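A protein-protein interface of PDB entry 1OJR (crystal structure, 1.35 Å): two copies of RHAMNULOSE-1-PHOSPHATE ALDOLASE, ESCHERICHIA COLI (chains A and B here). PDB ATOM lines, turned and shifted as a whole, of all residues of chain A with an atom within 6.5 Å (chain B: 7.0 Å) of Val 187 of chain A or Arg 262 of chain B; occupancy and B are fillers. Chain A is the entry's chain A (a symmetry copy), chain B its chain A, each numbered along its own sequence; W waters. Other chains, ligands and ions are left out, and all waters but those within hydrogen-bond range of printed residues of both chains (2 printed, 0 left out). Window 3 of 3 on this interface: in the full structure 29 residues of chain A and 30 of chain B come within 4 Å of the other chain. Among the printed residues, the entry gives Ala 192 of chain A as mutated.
The side-chain hydroxyl of Thr 170 of chain B sits at hydrogen-bond distance from the indole nitrogen of Trp 185 of chain A, at 2.9 Å. NH2 of Arg 262 of chain B is in hydrogen-bond range of O of Gly 189 of chain A, at 3.2 Å.
OE2 of Glu 117 of chain A sits at hydrogen-bond distance from N of Gly 189 of chain A, at 3.0 Å. The side-chain hydroxyl (OG1) of Thr 190 of chain A sits close to the backbone NH (N) of Ala 192 of chain A, 3.5 Å away. N of Ile 193 of chain A is in hydrogen-bond range of OG1 of Thr 190 of chain A (3.0 Å). O of Val 187 of chain A lies within hydrogen-bond range of OG1 of Thr 190 of chain A (3.3 Å).
Among the printed residues, pairs that only touch across the chains: Trp 185 of chain A with Glu 255 of chain B, Val 187 of chain A with Arg 262 of chain B, Pro 188 of chain A with Leu 259 of chain B, Pro 188 of chain A with Phe 263 of chain B and Thr 190 of chain A with Arg 262 of chain B.
Val 187 of chain A touches just one residue of chain B: Arg 262. Arg 262 of chain B touches three residues of chain A. Of the printed residues of chain B, Pro 188 of chain A touches Leu 259 (3.7 Å) and Phe 263 (3.8 Å). Of the printed residues of chain A, Thr 170 of chain B touches Trp 185 (2.9 Å). The nearest residue of chain B that does not touch Val 187 of chain A is Ala 258 of chain B (4.1 Å). The nearest residue of chain A that does not touch Arg 262 of chain B is Pro 188 of chain A (4.6 Å).
Of the 11 printed residues of chain A, 5 touch a printed residue of chain B. Printed residues of chain A that touch a printed residue of chain B: Trp 185, Val 187, Pro 188, Gly 189 and Thr 190.
No position is printed for both chains.
Water W2 lies within hydrogen-bond range of NE of Arg 262 of chain B (2.6 Å), O of Pro 188 of chain A (2.8 Å) and O of Gly 189 of chain A (3.3 Å). Water W1 lies within hydrogen-bond range of O of Trp 185 of chain A and OE1 of Glu 255 of chain B.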
ATOM      1  N   GLU A 117      -0.603  11.843   8.149  1.00  0.00           N
ATOM      2  CA  GLU A 117      -0.339  13.104   7.471  1.00  0.00           C
ATOM      3  C   GLU A 117      -1.263  14.197   7.999  1.00  0.00           C
ATOM      4  O   GLU A 117      -1.484  15.200   7.332  1.00  0.00           O
ATOM      5  CB  GLU A 117      -0.527  12.986   5.959  1.00  0.00           C
ATOM      6  CG  GLU A 117       0.378  11.991   5.259  1.00  0.00           C
ATOM      7  CD  GLU A 117       1.863  12.322   5.295  1.00  0.00           C
ATOM      8  OE1 GLU A 117       2.627  11.491   4.770  1.00  0.00           O
ATOM      9  OE2 GLU A 117       2.299  13.377   5.812  1.00  0.00           O
ATOM     10  N   TRP A 185      11.729  16.655  -2.625  1.00  0.00           N
ATOM     11  CA  TRP A 185      11.433  15.445  -1.877  1.00  0.00           C
ATOM     12  C   TRP A 185      11.674  15.697  -0.384  1.00  0.00           C
ATOM     13  O   TRP A 185      12.648  16.356  -0.003  1.00  0.00           O
ATOM     14  CB  TRP A 185      12.302  14.269  -2.347  1.00  0.00           C
ATOM     15  CG  TRP A 185      11.926  12.990  -1.672  1.00  0.00           C
ATOM     16  CD1 TRP A 185      11.026  12.075  -2.118  1.00  0.00           C
ATOM     17  CD2 TRP A 185      12.411  12.493  -0.414  1.00  0.00           C
ATOM     18  NE1 TRP A 185      10.919  11.039  -1.224  1.00  0.00           N
ATOM     19  CE2 TRP A 185      11.769  11.267  -0.172  1.00  0.00           C
ATOM     20  CE3 TRP A 185      13.323  12.968   0.540  1.00  0.00           C
ATOM     21  CZ2 TRP A 185      12.009  10.505   0.968  1.00  0.00           C
ATOM     22  CZ3 TRP A 185      13.561  12.206   1.675  1.00  0.00           C
ATOM     23  CH2 TRP A 185      12.903  10.989   1.881  1.00  0.00           C
ATOM     24  N   MET A 186      10.766  15.203   0.451  1.00  0.00           N
ATOM     25  CA  MET A 186      10.904  15.302   1.902  1.00  0.00           C
ATOM     26  C   MET A 186      10.382  14.028   2.544  1.00  0.00           C
ATOM     27  O   MET A 186       9.539  13.333   1.983  1.00  0.00           O
ATOM     28  CB  MET A 186      10.122  16.501   2.459  1.00  0.00           C
ATOM     29  CG  MET A 186      10.638  17.848   2.002  1.00  0.00           C
ATOM     30  SD  MET A 186       9.608  19.236   2.533  1.00  0.00           S
ATOM     31  CE  MET A 186       9.906  19.245   4.306  1.00  0.00           C
ATOM     32  N   VAL A 187      10.885  13.721   3.730  1.00  0.00           N
ATOM     33  CA  VAL A 187      10.410  12.577   4.490  1.00  0.00           C
ATOM     34  C   VAL A 187       8.935  12.825   4.817  1.00  0.00           C
ATOM     35  O   VAL A 187       8.588  13.877   5.340  1.00  0.00           O
ATOM     36  CB  VAL A 187      11.222  12.417   5.790  1.00  0.00           C
ATOM     37  CG1 VAL A 187      10.641  11.328   6.652  1.00  0.00           C
ATOM     38  CG2 VAL A 187      12.688  12.123   5.480  1.00  0.00           C
ATOM     39  N   PRO A 188       8.052  11.882   4.495  1.00  0.00           N
ATOM     40  CA  PRO A 188       6.620  12.074   4.733  1.00  0.00           C
ATOM     41  C   PRO A 188       6.214  11.841   6.188  1.00  0.00           C
ATOM     42  O   PRO A 188       6.972  11.257   6.956  1.00  0.00           O
ATOM     43  CB  PRO A 188       5.981  11.029   3.821  1.00  0.00           C
ATOM     44  CG  PRO A 188       6.979   9.941   3.740  1.00  0.00           C
ATOM     45  CD  PRO A 188       8.335  10.578   3.870  1.00  0.00           C
ATOM     46  N   GLY A 189       5.029  12.310   6.556  1.00  0.00           N
ATOM     47  CA  GLY A 189       4.493  12.086   7.885  1.00  0.00           C
ATOM     48  C   GLY A 189       5.053  12.986   8.966  1.00  0.00           C
ATOM     49  O   GLY A 189       4.911  12.689  10.145  1.00  0.00           O
ATOM     50  N   THR A 190       5.674  14.090   8.568  1.00  0.00           N
ATOM     51  CA  THR A 190       6.312  14.992   9.518  1.00  0.00           C
ATOM     52  C   THR A 190       5.624  16.339   9.588  1.00  0.00           C
ATOM     53  O   THR A 190       4.837  16.705   8.715  1.00  0.00           O
ATOM     54  CB  THR A 190       7.768  15.263   9.107  1.00  0.00           C
ATOM     55  OG1 THR A 190       7.794  15.910   7.824  1.00  0.00           O
ATOM     56  CG2 THR A 190       8.568  13.976   8.922  1.00  0.00           C
ATOM     57  N   ASP A 191       5.944  17.086  10.635  1.00  0.00           N
ATOM     58  CA  ASP A 191       5.488  18.455  10.739  1.00  0.00           C
ATOM     59  C   ASP A 191       6.122  19.284   9.626  1.00  0.00           C
ATOM     60  O   ASP A 191       5.475  20.150   9.054  1.00  0.00           O
ATOM     61  CB  ASP A 191       5.855  19.035  12.105  1.00  0.00           C
ATOM     62  CG  ASP A 191       5.040  18.432  13.215  1.00  0.00           C
ATOM     63  OD1 ASP A 191       5.636  17.898  14.181  1.00  0.00           O
ATOM     64  OD2 ASP A 191       3.793  18.448  13.198  1.00  0.00           O
ATOM     65  N   ALA A 192       7.393  19.029   9.323  1.00  0.00           N
ATOM     66  CA  ALA A 192       8.082  19.793   8.291  1.00  0.00           C
ATOM     67  C   ALA A 192       7.409  19.675   6.921  1.00  0.00           C
ATOM     68  O   ALA A 192       7.211  20.679   6.239  1.00  0.00           O
ATOM     69  CB  ALA A 192       9.532  19.360   8.182  1.00  0.00           C
ATOM     70  N   ILE A 193       7.087  18.458   6.499  1.00  0.00           N
ATOM     71  CA  ILE A 193       6.464  18.300   5.183  1.00  0.00           C
ATOM     72  C   ILE A 193       5.058  18.892   5.205  1.00  0.00           C
ATOM     73  O   ILE A 193       4.585  19.400   4.191  1.00  0.00           O
ATOM     74  CB  ILE A 193       6.491  16.828   4.683  1.00  0.00           C
ATOM     75  CG1 ILE A 193       6.360  16.802   3.148  1.00  0.00           C
ATOM     76  CG2 ILE A 193       5.406  15.994   5.356  1.00  0.00           C
ATOM     77  CD1 ILE A 193       6.474  15.414   2.527  1.00  0.00           C
ATOM     78  N   TRP A 209       4.367  16.068  -4.388  1.00  0.00           N
ATOM     79  CA  TRP A 209       5.425  15.497  -3.583  1.00  0.00           C
ATOM     80  C   TRP A 209       6.189  14.584  -4.540  1.00  0.00           C
ATOM     81  O   TRP A 209       5.693  13.518  -4.901  1.00  0.00           O
ATOM     82  CB  TRP A 209       4.810  14.681  -2.445  1.00  0.00           C
ATOM     83  CG  TRP A 209       4.269  15.471  -1.296  1.00  0.00           C
ATOM     84  CD1 TRP A 209       4.112  16.826  -1.218  1.00  0.00           C
ATOM     85  CD2 TRP A 209       3.836  14.946  -0.038  1.00  0.00           C
ATOM     86  NE1 TRP A 209       3.592  17.172   0.009  1.00  0.00           N
ATOM     87  CE2 TRP A 209       3.432  16.038   0.759  1.00  0.00           C
ATOM     88  CE3 TRP A 209       3.765  13.661   0.505  1.00  0.00           C
ATOM     89  CZ2 TRP A 209       2.961  15.879   2.062  1.00  0.00           C
ATOM     90  CZ3 TRP A 209       3.291  13.502   1.792  1.00  0.00           C
ATOM     91  CH2 TRP A 209       2.908  14.611   2.564  1.00  0.00           C
ATOM     92  N   THR B 170       7.973   6.422  -2.856  1.00  0.00           N
ATOM     93  CA  THR B 170       8.595   6.734  -1.580  1.00  0.00           C
ATOM     94  C   THR B 170       8.341   5.696  -0.492  1.00  0.00           C
ATOM     95  O   THR B 170       9.250   5.333   0.248  1.00  0.00           O
ATOM     96  CB  THR B 170       8.142   8.125  -1.123  1.00  0.00           C
ATOM     97  OG1 THR B 170       8.813   9.118  -1.916  1.00  0.00           O
ATOM     98  CG2 THR B 170       8.586   8.408   0.310  1.00  0.00           C
ATOM     99  N   GLU B 255      18.410  10.320   0.814  1.00  0.00           N
ATOM    100  CA  GLU B 255      16.983  10.407   1.105  1.00  0.00           C
ATOM    101  C   GLU B 255      16.450   9.067   1.628  1.00  0.00           C
ATOM    102  O   GLU B 255      15.701   9.020   2.606  1.00  0.00           O
ATOM    103  CB  GLU B 255      16.229  10.906  -0.128  1.00  0.00           C
ATOM    104  CG  GLU B 255      16.503  12.384  -0.372  1.00  0.00           C
ATOM    105  CD  GLU B 255      16.063  12.902  -1.725  1.00  0.00           C
ATOM    106  OE1 GLU B 255      15.923  14.139  -1.845  1.00  0.00           O
ATOM    107  OE2 GLU B 255      15.874  12.104  -2.661  1.00  0.00           O
ATOM    108  N   LEU B 256      16.872   7.975   1.009  1.00  0.00           N
ATOM    109  CA  LEU B 256      16.486   6.649   1.468  1.00  0.00           C
ATOM    110  C   LEU B 256      16.962   6.391   2.892  1.00  0.00           C
ATOM    111  O   LEU B 256      16.238   5.806   3.701  1.00  0.00           O
ATOM    112  CB  LEU B 256      17.035   5.583   0.527  1.00  0.00           C
ATOM    113  CG  LEU B 256      16.393   5.575  -0.867  1.00  0.00           C
ATOM    114  CD1 LEU B 256      17.229   4.702  -1.794  1.00  0.00           C
ATOM    115  CD2 LEU B 256      14.950   5.096  -0.846  1.00  0.00           C
ATOM    116  N   ILE B 257      18.183   6.821   3.203  1.00  0.00           N
ATOM    117  CA  ILE B 257      18.710   6.659   4.551  1.00  0.00           C
ATOM    118  C   ILE B 257      17.862   7.442   5.560  1.00  0.00           C
ATOM    119  O   ILE B 257      17.500   6.912   6.616  1.00  0.00           O
ATOM    120  CB  ILE B 257      20.185   7.100   4.619  1.00  0.00           C
ATOM    121  CG1 ILE B 257      21.063   6.098   3.864  1.00  0.00           C
ATOM    122  CG2 ILE B 257      20.630   7.215   6.067  1.00  0.00           C
ATOM    123  CD1 ILE B 257      22.482   6.561   3.622  1.00  0.00           C
ATOM    124  N   ALA B 258      17.533   8.692   5.229  1.00  0.00           N
ATOM    125  CA  ALA B 258      16.710   9.525   6.107  1.00  0.00           C
ATOM    126  C   ALA B 258      15.332   8.894   6.308  1.00  0.00           C
ATOM    127  O   ALA B 258      14.766   8.926   7.394  1.00  0.00           O
ATOM    128  CB  ALA B 258      16.573  10.921   5.535  1.00  0.00           C
ATOM    129  N   LEU B 259      14.777   8.358   5.230  1.00  0.00           N
ATOM    130  CA  LEU B 259      13.491   7.693   5.281  1.00  0.00           C
ATOM    131  C   LEU B 259      13.527   6.485   6.230  1.00  0.00           C
ATOM    132  O   LEU B 259      12.648   6.310   7.075  1.00  0.00           O
ATOM    133  CB  LEU B 259      13.110   7.273   3.863  1.00  0.00           C
ATOM    134  CG  LEU B 259      11.735   6.674   3.640  1.00  0.00           C
ATOM    135  CD1 LEU B 259      10.629   7.672   3.966  1.00  0.00           C
ATOM    136  CD2 LEU B 259      11.657   6.214   2.201  1.00  0.00           C
ATOM    137  N   GLY B 260      14.562   5.662   6.100  1.00  0.00           N
ATOM    138  CA  GLY B 260      14.723   4.507   6.962  1.00  0.00           C
ATOM    139  C   GLY B 260      14.857   4.897   8.428  1.00  0.00           C
ATOM    140  O   GLY B 260      14.267   4.275   9.302  1.00  0.00           O
ATOM    141  N   LYS B 261      15.626   5.941   8.697  1.00  0.00           N
ATOM    142  CA  LYS B 261      15.819   6.400  10.071  1.00  0.00           C
ATOM    143  C   LYS B 261      14.496   6.859  10.685  1.00  0.00           C
ATOM    144  O   LYS B 261      14.165   6.506  11.815  1.00  0.00           O
ATOM    145  CB  LYS B 261      16.851   7.529  10.124  1.00  0.00           C
ATOM    146  CG  LYS B 261      18.298   7.056  10.067  1.00  0.00           C
ATOM    147  CD  LYS B 261      19.245   8.227   9.828  1.00  0.00           C
ATOM    148  CE  LYS B 261      20.694   7.784   9.692  1.00  0.00           C
ATOM    149  NZ  LYS B 261      21.562   8.896   9.208  1.00  0.00           N
ATOM    150  N   ARG B 262      13.730   7.635   9.928  1.00  0.00           N
ATOM    151  CA  ARG B 262      12.459   8.156  10.414  1.00  0.00           C
ATOM    152  C   ARG B 262      11.473   7.048  10.750  1.00  0.00           C
ATOM    153  O   ARG B 262      10.779   7.109  11.771  1.00  0.00           O
ATOM    154  CB  ARG B 262      11.841   9.081   9.362  1.00  0.00           C
ATOM    155  CG  ARG B 262      10.435   9.522   9.673  1.00  0.00           C
ATOM    156  CD  ARG B 262      10.328  10.426  10.872  1.00  0.00           C
ATOM    157  NE  ARG B 262       8.942  10.810  11.116  1.00  0.00           N
ATOM    158  CZ  ARG B 262       8.552  11.703  12.014  1.00  0.00           C
ATOM    159  NH1 ARG B 262       9.442  12.329  12.777  1.00  0.00           N
ATOM    160  NH2 ARG B 262       7.262  11.976  12.146  1.00  0.00           N
ATOM    161  N   PHE B 263      11.412   6.033   9.895  1.00  0.00           N
ATOM    162  CA  PHE B 263      10.453   4.953  10.077  1.00  0.00           C
ATOM    163  C   PHE B 263      10.980   3.757  10.864  1.00  0.00           C
ATOM    164  O   PHE B 263      10.276   2.762  11.022  1.00  0.00           O
ATOM    165  CB  PHE B 263       9.870   4.541   8.723  1.00  0.00           C
ATOM    166  CG  PHE B 263       8.902   5.542   8.194  1.00  0.00           C
ATOM    167  CD1 PHE B 263       9.336   6.604   7.418  1.00  0.00           C
ATOM    168  CD2 PHE B 263       7.564   5.469   8.538  1.00  0.00           C
ATOM    169  CE1 PHE B 263       8.440   7.555   6.963  1.00  0.00           C
ATOM    170  CE2 PHE B 263       6.663   6.413   8.085  1.00  0.00           C
ATOM    171  CZ  PHE B 263       7.104   7.462   7.302  1.00  0.00           C
ATOM    172  N   GLY B 264      12.203   3.873  11.375  1.00  0.00           N
ATOM    173  CA  GLY B 264      12.793   2.843  12.217  1.00  0.00           C
ATOM    174  C   GLY B 264      13.005   1.505  11.543  1.00  0.00           C
ATOM    175  O   GLY B 264      12.803   0.461  12.154  1.00  0.00           O
ATOM    176  N   VAL B 265      13.411   1.528  10.278  1.00  0.00           N
ATOM    177  CA  VAL B 265      13.686   0.297   9.546  1.00  0.00           C
ATOM    178  C   VAL B 265      15.131   0.338   9.067  1.00  0.00           C
ATOM    179  O   VAL B 265      15.674   1.418   8.840  1.00  0.00           O
ATOM    180  CB  VAL B 265      12.720   0.090   8.345  1.00  0.00           C
ATOM    181  CG1 VAL B 265      11.278  -0.056   8.821  1.00  0.00           C
ATOM    182  CG2 VAL B 265      12.837   1.214   7.336  1.00  0.00           C
HETATM  183  O   HOH W   1      15.135  17.113  -0.977  1.00  0.00           O
HETATM  184  O   HOH W   2       6.981  10.163   9.545  1.00  0.00           O
